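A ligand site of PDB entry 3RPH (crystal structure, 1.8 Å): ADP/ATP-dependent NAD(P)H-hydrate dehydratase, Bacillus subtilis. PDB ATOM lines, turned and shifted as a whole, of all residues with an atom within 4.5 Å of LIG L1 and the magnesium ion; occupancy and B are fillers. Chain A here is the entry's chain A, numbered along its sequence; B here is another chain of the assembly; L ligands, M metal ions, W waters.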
ATOM      1  N   ASP A 131     -21.067 -27.845  -3.573  1.00  0.00           N
ATOM      2  CA  ASP A 131     -20.437 -26.918  -2.615  1.00  0.00           C
ATOM      3  C   ASP A 131     -21.049 -27.104  -1.248  1.00  0.00           C
ATOM      4  O   ASP A 131     -22.149 -27.641  -1.121  1.00  0.00           O
ATOM      5  CB  ASP A 131     -20.620 -25.456  -3.118  1.00  0.00           C
ATOM      6  CG  ASP A 131     -19.898 -24.443  -2.272  1.00  0.00           C
ATOM      7  OD1 ASP A 131     -18.847 -24.793  -1.681  1.00  0.00           O
ATOM      8  OD2 ASP A 131     -20.367 -23.272  -2.238  1.00  0.00           O
ATOM      9  N   HIS A 152     -13.412 -25.467   0.724  1.00  0.00           N
ATOM     10  CA  HIS A 152     -12.331 -24.874   1.458  1.00  0.00           C
ATOM     11  C   HIS A 152     -11.633 -25.976   2.229  1.00  0.00           C
ATOM     12  O   HIS A 152     -12.105 -27.128   2.259  1.00  0.00           O
ATOM     13  CB  HIS A 152     -12.756 -23.697   2.333  1.00  0.00           C
ATOM     14  CG  HIS A 152     -13.689 -24.033   3.429  1.00  0.00           C
ATOM     15  ND1 HIS A 152     -13.417 -24.996   4.376  1.00  0.00           N
ATOM     16  CD2 HIS A 152     -14.896 -23.509   3.742  1.00  0.00           C
ATOM     17  CE1 HIS A 152     -14.427 -25.050   5.245  1.00  0.00           C
ATOM     18  NE2 HIS A 152     -15.329 -24.145   4.893  1.00  0.00           N
ATOM     19  N   GLU A 155     -13.645 -28.281   4.461  1.00  0.00           N
ATOM     20  CA  GLU A 155     -14.476 -29.154   3.689  1.00  0.00           C
ATOM     21  C   GLU A 155     -13.652 -30.259   3.025  1.00  0.00           C
ATOM     22  O   GLU A 155     -14.117 -31.399   2.914  1.00  0.00           O
ATOM     23  CB  GLU A 155     -15.240 -28.331   2.663  1.00  0.00           C
ATOM     24  CG  GLU A 155     -16.383 -27.537   3.336  1.00  0.00           C
ATOM     25  CD  GLU A 155     -16.933 -26.387   2.539  1.00  0.00           C
ATOM     26  OE1 GLU A 155     -16.282 -25.914   1.588  1.00  0.00           O
ATOM     27  OE2 GLU A 155     -18.018 -25.882   2.981  1.00  0.00           O
ATOM     28  N   LYS A 189     -10.060 -24.066  -2.281  1.00  0.00           N
ATOM     29  CA  LYS A 189     -10.064 -22.644  -1.978  1.00  0.00           C
ATOM     30  C   LYS A 189      -8.977 -22.213  -1.033  1.00  0.00           C
ATOM     31  O   LYS A 189      -8.374 -23.052  -0.351  1.00  0.00           O
ATOM     32  CB  LYS A 189     -11.381 -22.290  -1.366  1.00  0.00           C
ATOM     33  CG  LYS A 189     -12.550 -22.404  -2.298  1.00  0.00           C
ATOM     34  CD  LYS A 189     -13.819 -22.445  -1.404  1.00  0.00           C
ATOM     35  CE  LYS A 189     -14.980 -22.139  -2.217  1.00  0.00           C
ATOM     36  NZ  LYS A 189     -16.278 -22.595  -1.544  1.00  0.00           N
ATOM     37  N   GLY A 190      -8.752 -20.891  -1.030  1.00  0.00           N
ATOM     38  CA  GLY A 190      -7.742 -20.249  -0.249  1.00  0.00           C
ATOM     39  C   GLY A 190      -6.924 -19.272  -1.082  1.00  0.00           C
ATOM     40  O   GLY A 190      -7.102 -19.141  -2.292  1.00  0.00           O
ATOM     41  N   ASN A 191      -6.018 -18.576  -0.419  1.00  0.00           N
ATOM     42  CA  ASN A 191      -4.949 -17.894  -1.120  1.00  0.00           C
ATOM     43  C   ASN A 191      -4.356 -18.907  -2.108  1.00  0.00           C
ATOM     44  O   ASN A 191      -4.119 -20.053  -1.734  1.00  0.00           O
ATOM     45  CB  ASN A 191      -3.904 -17.387  -0.110  1.00  0.00           C
ATOM     46  CG  ASN A 191      -2.726 -16.676  -0.780  1.00  0.00           C
ATOM     47  OD1 ASN A 191      -2.886 -15.820  -1.623  1.00  0.00           O
ATOM     48  ND2 ASN A 191      -1.490 -17.087  -0.388  1.00  0.00           N
ATOM     49  N   THR A 193      -5.796 -20.378  -4.837  1.00  0.00           N
ATOM     50  CA  THR A 193      -6.778 -21.432  -5.004  1.00  0.00           C
ATOM     51  C   THR A 193      -6.203 -22.391  -6.042  1.00  0.00           C
ATOM     52  O   THR A 193      -5.656 -21.945  -7.061  1.00  0.00           O
ATOM     53  CB  THR A 193      -8.148 -20.843  -5.459  1.00  0.00           C
ATOM     54  OG1 THR A 193      -8.777 -20.264  -4.289  1.00  0.00           O
ATOM     55  CG2 THR A 193      -9.059 -21.923  -6.108  1.00  0.00           C
ATOM     56  N   GLY A 208      -7.063 -12.262  -5.967  1.00  0.00           N
ATOM     57  CA  GLY A 208      -7.711 -12.352  -4.665  1.00  0.00           C
ATOM     58  C   GLY A 208      -6.858 -11.897  -3.515  1.00  0.00           C
ATOM     59  O   GLY A 208      -5.638 -11.720  -3.628  1.00  0.00           O
ATOM     60  N   ASN A 209      -7.529 -11.642  -2.404  1.00  0.00           N
ATOM     61  CA  ASN A 209      -6.844 -11.165  -1.210  1.00  0.00           C
ATOM     62  C   ASN A 209      -7.728 -11.365  -0.002  1.00  0.00           C
ATOM     63  O   ASN A 209      -8.808 -12.016  -0.106  1.00  0.00           O
ATOM     64  CB  ASN A 209      -6.424  -9.700  -1.356  1.00  0.00           C
ATOM     65  CG  ASN A 209      -7.625  -8.782  -1.604  1.00  0.00           C
ATOM     66  OD1 ASN A 209      -8.681  -8.971  -1.010  1.00  0.00           O
ATOM     67  ND2 ASN A 209      -7.444  -7.783  -2.469  1.00  0.00           N
ATOM     68  N   GLY A 210      -7.242 -10.910   1.143  1.00  0.00           N
ATOM     69  CA  GLY A 210      -7.956 -11.157   2.398  1.00  0.00           C
ATOM     70  C   GLY A 210      -9.322 -10.532   2.518  1.00  0.00           C
ATOM     71  O   GLY A 210     -10.055 -10.838   3.481  1.00  0.00           O
ATOM     72  N   LEU A 212     -11.633 -11.323   0.823  1.00  0.00           N
ATOM     73  CA  LEU A 212     -12.446 -12.542   0.597  1.00  0.00           C
ATOM     74  C   LEU A 212     -12.617 -13.432   1.815  1.00  0.00           C
ATOM     75  O   LEU A 212     -13.436 -14.342   1.790  1.00  0.00           O
ATOM     76  CB  LEU A 212     -11.871 -13.360  -0.575  1.00  0.00           C
ATOM     77  CG  LEU A 212     -11.955 -12.677  -1.938  1.00  0.00           C
ATOM     78  CD1 LEU A 212     -11.188 -13.513  -2.985  1.00  0.00           C
ATOM     79  CD2 LEU A 212     -13.413 -12.372  -2.443  1.00  0.00           C
ATOM     80  N   ALA A 213     -11.885 -13.160   2.882  1.00  0.00           N
ATOM     81  CA  ALA A 213     -11.847 -14.022   4.076  1.00  0.00           C
ATOM     82  C   ALA A 213     -12.969 -13.644   5.002  1.00  0.00           C
ATOM     83  O   ALA A 213     -12.750 -13.161   6.106  1.00  0.00           O
ATOM     84  CB  ALA A 213     -10.456 -13.866   4.805  1.00  0.00           C
ATOM     85  N   GLY A 216     -19.658 -15.948   3.001  1.00  0.00           N
ATOM     86  CA  GLY A 216     -20.447 -15.748   1.822  1.00  0.00           C
ATOM     87  C   GLY A 216     -19.697 -15.666   0.534  1.00  0.00           C
ATOM     88  O   GLY A 216     -20.287 -15.852  -0.536  1.00  0.00           O
ATOM     89  N   THR A 217     -18.390 -15.394   0.584  1.00  0.00           N
ATOM     90  CA  THR A 217     -17.657 -15.217  -0.643  1.00  0.00           C
ATOM     91  C   THR A 217     -17.646 -16.487  -1.494  1.00  0.00           C
ATOM     92  O   THR A 217     -17.663 -16.384  -2.744  1.00  0.00           O
ATOM     93  CB  THR A 217     -16.274 -14.671  -0.378  1.00  0.00           C
ATOM     94  OG1 THR A 217     -15.558 -15.573   0.474  1.00  0.00           O
ATOM     95  CG2 THR A 217     -16.367 -13.261   0.247  1.00  0.00           C
ATOM     96  N   GLY A 218     -17.592 -17.668  -0.893  1.00  0.00           N
ATOM     97  CA  GLY A 218     -17.619 -18.862  -1.671  1.00  0.00           C
ATOM     98  C   GLY A 218     -18.996 -19.115  -2.300  1.00  0.00           C
ATOM     99  O   GLY A 218     -19.079 -19.850  -3.303  1.00  0.00           O
ATOM    100  N   ASP A 219     -20.071 -18.625  -1.668  1.00  0.00           N
ATOM    101  CA  ASP A 219     -21.409 -18.754  -2.245  1.00  0.00           C
ATOM    102  C   ASP A 219     -21.527 -17.975  -3.550  1.00  0.00           C
ATOM    103  O   ASP A 219     -22.002 -18.460  -4.573  1.00  0.00           O
ATOM    104  CB  ASP A 219     -22.487 -18.349  -1.231  1.00  0.00           C
ATOM    105  CG  ASP A 219     -22.426 -19.169   0.039  1.00  0.00           C
ATOM    106  OD1 ASP A 219     -22.156 -20.406   0.014  1.00  0.00           O
ATOM    107  OD2 ASP A 219     -22.653 -18.513   1.090  1.00  0.00           O
ATOM    108  N   LEU A 221     -18.942 -17.285  -5.413  1.00  0.00           N
ATOM    109  CA  LEU A 221     -18.106 -18.045  -6.354  1.00  0.00           C
ATOM    110  C   LEU A 221     -18.900 -19.184  -6.994  1.00  0.00           C
ATOM    111  O   LEU A 221     -18.846 -19.411  -8.194  1.00  0.00           O
ATOM    112  CB  LEU A 221     -16.856 -18.569  -5.689  1.00  0.00           C
ATOM    113  CG  LEU A 221     -15.980 -19.445  -6.611  1.00  0.00           C
ATOM    114  CD1 LEU A 221     -15.478 -18.641  -7.866  1.00  0.00           C
ATOM    115  CD2 LEU A 221     -14.768 -20.062  -5.852  1.00  0.00           C
ATOM    116  N   HIS A 246     -13.523 -13.709  -9.795  1.00  0.00           N
ATOM    117  CA  HIS A 246     -13.909 -13.576  -8.387  1.00  0.00           C
ATOM    118  C   HIS A 246     -12.815 -12.902  -7.562  1.00  0.00           C
ATOM    119  O   HIS A 246     -13.074 -11.905  -6.868  1.00  0.00           O
ATOM    120  CB  HIS A 246     -14.293 -14.968  -7.877  1.00  0.00           C
ATOM    121  CG  HIS A 246     -14.673 -15.087  -6.412  1.00  0.00           C
ATOM    122  ND1 HIS A 246     -13.782 -15.537  -5.455  1.00  0.00           N
ATOM    123  CD2 HIS A 246     -15.869 -14.943  -5.785  1.00  0.00           C
ATOM    124  CE1 HIS A 246     -14.418 -15.637  -4.296  1.00  0.00           C
ATOM    125  NE2 HIS A 246     -15.674 -15.262  -4.458  1.00  0.00           N
ATOM    126  N   ASP B  22      -4.095 -10.330   6.236  1.00  0.00           N
ATOM    127  CA  ASP B  22      -3.016 -10.978   5.475  1.00  0.00           C
ATOM    128  C   ASP B  22      -3.520 -11.827   4.308  1.00  0.00           C
ATOM    129  O   ASP B  22      -4.584 -12.414   4.396  1.00  0.00           O
ATOM    130  CB  ASP B  22      -2.188 -11.898   6.392  1.00  0.00           C
ATOM    131  CG  ASP B  22      -1.299 -11.137   7.368  1.00  0.00           C
ATOM    132  OD1 ASP B  22      -0.971  -9.922   7.139  1.00  0.00           O
ATOM    133  OD2 ASP B  22      -0.870 -11.775   8.347  1.00  0.00           O
ATOM    134  N   ALA B  23      -2.685 -11.945   3.282  1.00  0.00           N
ATOM    135  CA  ALA B  23      -2.954 -12.814   2.137  1.00  0.00           C
ATOM    136  C   ALA B  23      -3.270 -14.232   2.599  1.00  0.00           C
ATOM    137  O   ALA B  23      -4.164 -14.880   2.052  1.00  0.00           O
ATOM    138  CB  ALA B  23      -1.770 -12.828   1.189  1.00  0.00           C
ATOM    139  N   SER B  25      -4.860 -15.896   5.042  1.00  0.00           N
ATOM    140  CA  SER B  25      -5.912 -15.856   6.076  1.00  0.00           C
ATOM    141  C   SER B  25      -7.228 -16.304   5.483  1.00  0.00           C
ATOM    142  O   SER B  25      -7.411 -16.324   4.263  1.00  0.00           O
ATOM    143  CB  SER B  25      -6.045 -14.446   6.734  1.00  0.00           C
ATOM    144  OG  SER B  25      -6.486 -13.435   5.818  1.00  0.00           O
ATOM    145  N   HIS B  26      -8.153 -16.719   6.329  1.00  0.00           N
ATOM    146  CA  HIS B  26      -9.457 -17.133   5.853  1.00  0.00           C
ATOM    147  C   HIS B  26     -10.469 -16.683   6.874  1.00  0.00           C
ATOM    148  O   HIS B  26     -10.101 -16.104   7.881  1.00  0.00           O
ATOM    149  CB  HIS B  26      -9.506 -18.642   5.675  1.00  0.00           C
ATOM    150  CG  HIS B  26      -9.094 -19.372   6.909  1.00  0.00           C
ATOM    151  ND1 HIS B  26      -9.999 -19.783   7.868  1.00  0.00           N
ATOM    152  CD2 HIS B  26      -7.873 -19.747   7.353  1.00  0.00           C
ATOM    153  CE1 HIS B  26      -9.351 -20.385   8.852  1.00  0.00           C
ATOM    154  NE2 HIS B  26      -8.058 -20.379   8.561  1.00  0.00           N
ATOM    155  N   LYS B  27     -11.750 -16.921   6.648  1.00  0.00           N
ATOM    156  CA  LYS B  27     -12.739 -16.405   7.585  1.00  0.00           C
ATOM    157  C   LYS B  27     -12.522 -16.844   9.066  1.00  0.00           C
ATOM    158  O   LYS B  27     -12.806 -16.086  10.027  1.00  0.00           O
ATOM    159  CB  LYS B  27     -14.137 -16.747   7.156  1.00  0.00           C
ATOM    160  CG  LYS B  27     -14.429 -18.273   7.134  1.00  0.00           C
ATOM    161  CD  LYS B  27     -15.683 -18.541   6.223  1.00  0.00           C
ATOM    162  CE  LYS B  27     -15.865 -20.051   5.992  1.00  0.00           C
ATOM    163  NZ  LYS B  27     -16.911 -20.380   4.973  1.00  0.00           N
HETATM  164  P1  LIG L   1     -16.004 -20.019   1.419  1.00  0.00           P
HETATM  165  O1  LIG L   1     -16.822 -18.747   1.603  1.00  0.00           O
HETATM  166  O2  LIG L   1     -15.236 -20.381   2.666  1.00  0.00           O
HETATM  167  O3  LIG L   1     -16.810 -21.124   0.762  1.00  0.00           O
HETATM  168  O4  LIG L   1     -15.048 -19.585   0.261  1.00  0.00           O
HETATM  169  C1  LIG L   1     -14.092 -18.544   0.488  1.00  0.00           C
HETATM  170  C2  LIG L   1     -13.713 -17.885  -0.817  1.00  0.00           C
HETATM  171  O5  LIG L   1     -12.884 -16.746  -0.537  1.00  0.00           O
HETATM  172  C3  LIG L   1     -12.898 -18.781  -1.727  1.00  0.00           C
HETATM  173  O6  LIG L   1     -13.046 -18.401  -3.105  1.00  0.00           O
HETATM  174  C4  LIG L   1     -11.468 -18.522  -1.242  1.00  0.00           C
HETATM  175  O7  LIG L   1     -10.420 -18.910  -2.138  1.00  0.00           O
HETATM  176  C5  LIG L   1     -11.541 -17.010  -1.021  1.00  0.00           C
HETATM  177  N1  LIG L   1     -10.591 -16.506  -0.051  1.00  0.00           N
HETATM  178  C6  LIG L   1     -10.707 -16.465   1.284  1.00  0.00           C
HETATM  179  N2  LIG L   1      -9.632 -15.871   1.884  1.00  0.00           N
HETATM  180  C7  LIG L   1      -8.813 -15.529   0.874  1.00  0.00           C
HETATM  181  C8  LIG L   1      -7.500 -14.894   0.785  1.00  0.00           C
HETATM  182  N3  LIG L   1      -6.957 -14.548   1.962  1.00  0.00           N
HETATM  183  N4  LIG L   1      -6.943 -14.706  -0.428  1.00  0.00           N
HETATM  184  C9  LIG L   1      -7.589 -15.069  -1.536  1.00  0.00           C
HETATM  185  N5  LIG L   1      -8.804 -15.687  -1.524  1.00  0.00           N
HETATM  186  C10 LIG L   1      -9.431 -15.935  -0.395  1.00  0.00           C
HETATM  187  P1  LG2 L   2     -19.818 -19.424   3.163  1.00  0.00           P
HETATM  188  O1  LG2 L   2     -19.168 -20.643   2.556  1.00  0.00           O
HETATM  189  O2  LG2 L   2     -19.276 -18.831   4.508  1.00  0.00           O
HETATM  190  O3  LG2 L   2     -21.374 -19.513   3.259  1.00  0.00           O
HETATM  191  O4  LG2 L   2     -19.449 -18.517   1.963  1.00  0.00           O
HETATM  192 MG    MG M   1     -18.434 -22.109   1.405  1.00  0.00          MG
HETATM  193  O   HOH W   1     -12.708 -20.224   3.496  1.00  0.00           O
HETATM  194  O   HOH W   2     -11.444 -19.284  -5.046  1.00  0.00           O
HETATM  195  O   HOH W   3     -15.468 -17.078   3.353  1.00  0.00           O
HETATM  196  O   HOH W   4      -4.502 -13.834  -1.188  1.00  0.00           O
HETATM  197  O   HOH W   5      -9.471 -17.084  -3.948  1.00  0.00           O
HETATM  198  O   HOH W   6     -17.765 -23.870   0.444  1.00  0.00           O
HETATM  199  O   HOH W   7     -18.085 -23.084   3.200  1.00  0.00           O
HETATM  200  O   HOH W   8     -19.823 -21.788  -0.163  1.00  0.00           O
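Residues that only touch the magnesium ion: Lys 189 (3.7 Å). Of the 23 residues printed, 1 comes within 4 Å of the magnesium ion. The nearest printed residue that does not touch the magnesium ion is Glu 155 (4.1 Å).
The side-chain amino group (NZ) of Lys 189 is in salt-bridge range of the side-chain carboxylate (OD1) of Asp 131 (3.4 Å). The side-chain hydroxyl (OG1) of Thr 193 lies within hydrogen-bond range of the backbone carbonyl oxygen (O) of Gly 190 (2.8 Å). OG of Ser 25 of chain B is in hydrogen-bond range of O of Asp 22 of chain B (2.6 Å). The backbone carbonyl oxygen (O) of Thr 217 is in hydrogen-bond range of a ring nitrogen (NE2) of His 246 (2.9 Å). OG1 of Thr 217 is in hydrogen-bond range of O of Leu 212 (2.8 Å). OE1 of Glu 155 sits at hydrogen-bond distance from N of His 152, at 3.0 Å.
The backbone carbonyl oxygen of Asn 209 sits close to a nitrogen (N4) of LIG L1, 3.3 Å away. O5 of LIG L1 lies close to O of Leu 212, 3.4 Å away. Merely in contact with LIG L1: His 246, His 152, Gly 210, Ala 213, Leu 221, Gly 208 and Asn 191. Hydrophobic or aromatic side chains that line LIG L1: His 152, Leu 212, Ala 213, Leu 221 and His 246. Of the 23 residues printed, 17 come within 4 Å of LIG L1. The nearest printed residue that does not touch LIG L1 is Asp 22 of chain B (4.01 Å).
Water W8 bridges the side-chain carboxylate (OD2) of Asp 131 (2.6 Å) and the side-chain carboxylate (OD1) of Asp 219 (2.7 Å). Water W6 lies within hydrogen-bond range of OD1 of Asp 131 (2.6 Å), OE1 of Glu 155 (2.8 Å) and NZ of Lys 189 (2.8 Å). Water W7 lies within hydrogen-bond range of the side-chain carboxylate of Glu 155 (2.8 Å), a ring nitrogen (NE2) of His 152 (3.4 Å) and the side-chain amino group of Lys 27 of chain B (3.4 Å). Water W2 lies within hydrogen-bond range of an oxygen (O6) of LIG L1 (2.7 Å) and the side-chain hydroxyl of Thr 193 (2.9 Å). Water W5 lies within hydrogen-bond range of O7 of LIG L1 (2.7 Å) and OG1 of Thr 193 (3.3 Å). Water W3 bridges O1 of LIG L1 (2.8 Å) and OG1 of Thr 217 (3.2 Å).
The magnesium ion is bound by O1 of LG2 L2 (2.0 Å), O3 of LIG L1 (2.0 Å), water W7 (2.1 Å), water W6 (2.1 Å) and water W8 (2.1 Å). The magnesium ion has five donor atoms within binding distance.
The side-chain amino group (NZ) of Lys 189 lies close to an oxygen (O3) of LIG L1, at 2.8 Å. A nitrogen (N3) of LIG L1 lies within hydrogen-bond range of the backbone carbonyl oxygen of Ala 23 of chain B, at 2.8 Å. An oxygen (O7) of LIG L1 is in hydrogen-bond range of the backbone NH (N) of Gly 190, 2.8 Å away. An oxygen (O7) of LIG L1 sits at hydrogen-bond distance from the backbone carbonyl oxygen (O) of Gly 190, at 3.3 Å. The backbone NH (N) of Gly 218 lies within hydrogen-bond range of an oxygen (O1) of LIG L1, 2.8 Å away. The side-chain amino group (NZ) of Lys 27 of chain B is in salt-bridge range of an oxygen (O2) of LIG L1, 2.9 Å away. The backbone carbonyl oxygen (O) of Ser 25 of chain B is in hydrogen-bond range of a nitrogen (N3) of LIG L1 (2.9 Å). An oxygen (O7) of LIG L1 sits at hydrogen-bond distance from the side-chain hydroxyl (OG1) of Thr 193 (3.0 Å). An oxygen (O5) of LIG L1 sits at hydrogen-bond distance from the side-chain hydroxyl (OG1) of Thr 217, at 3.1 Å.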
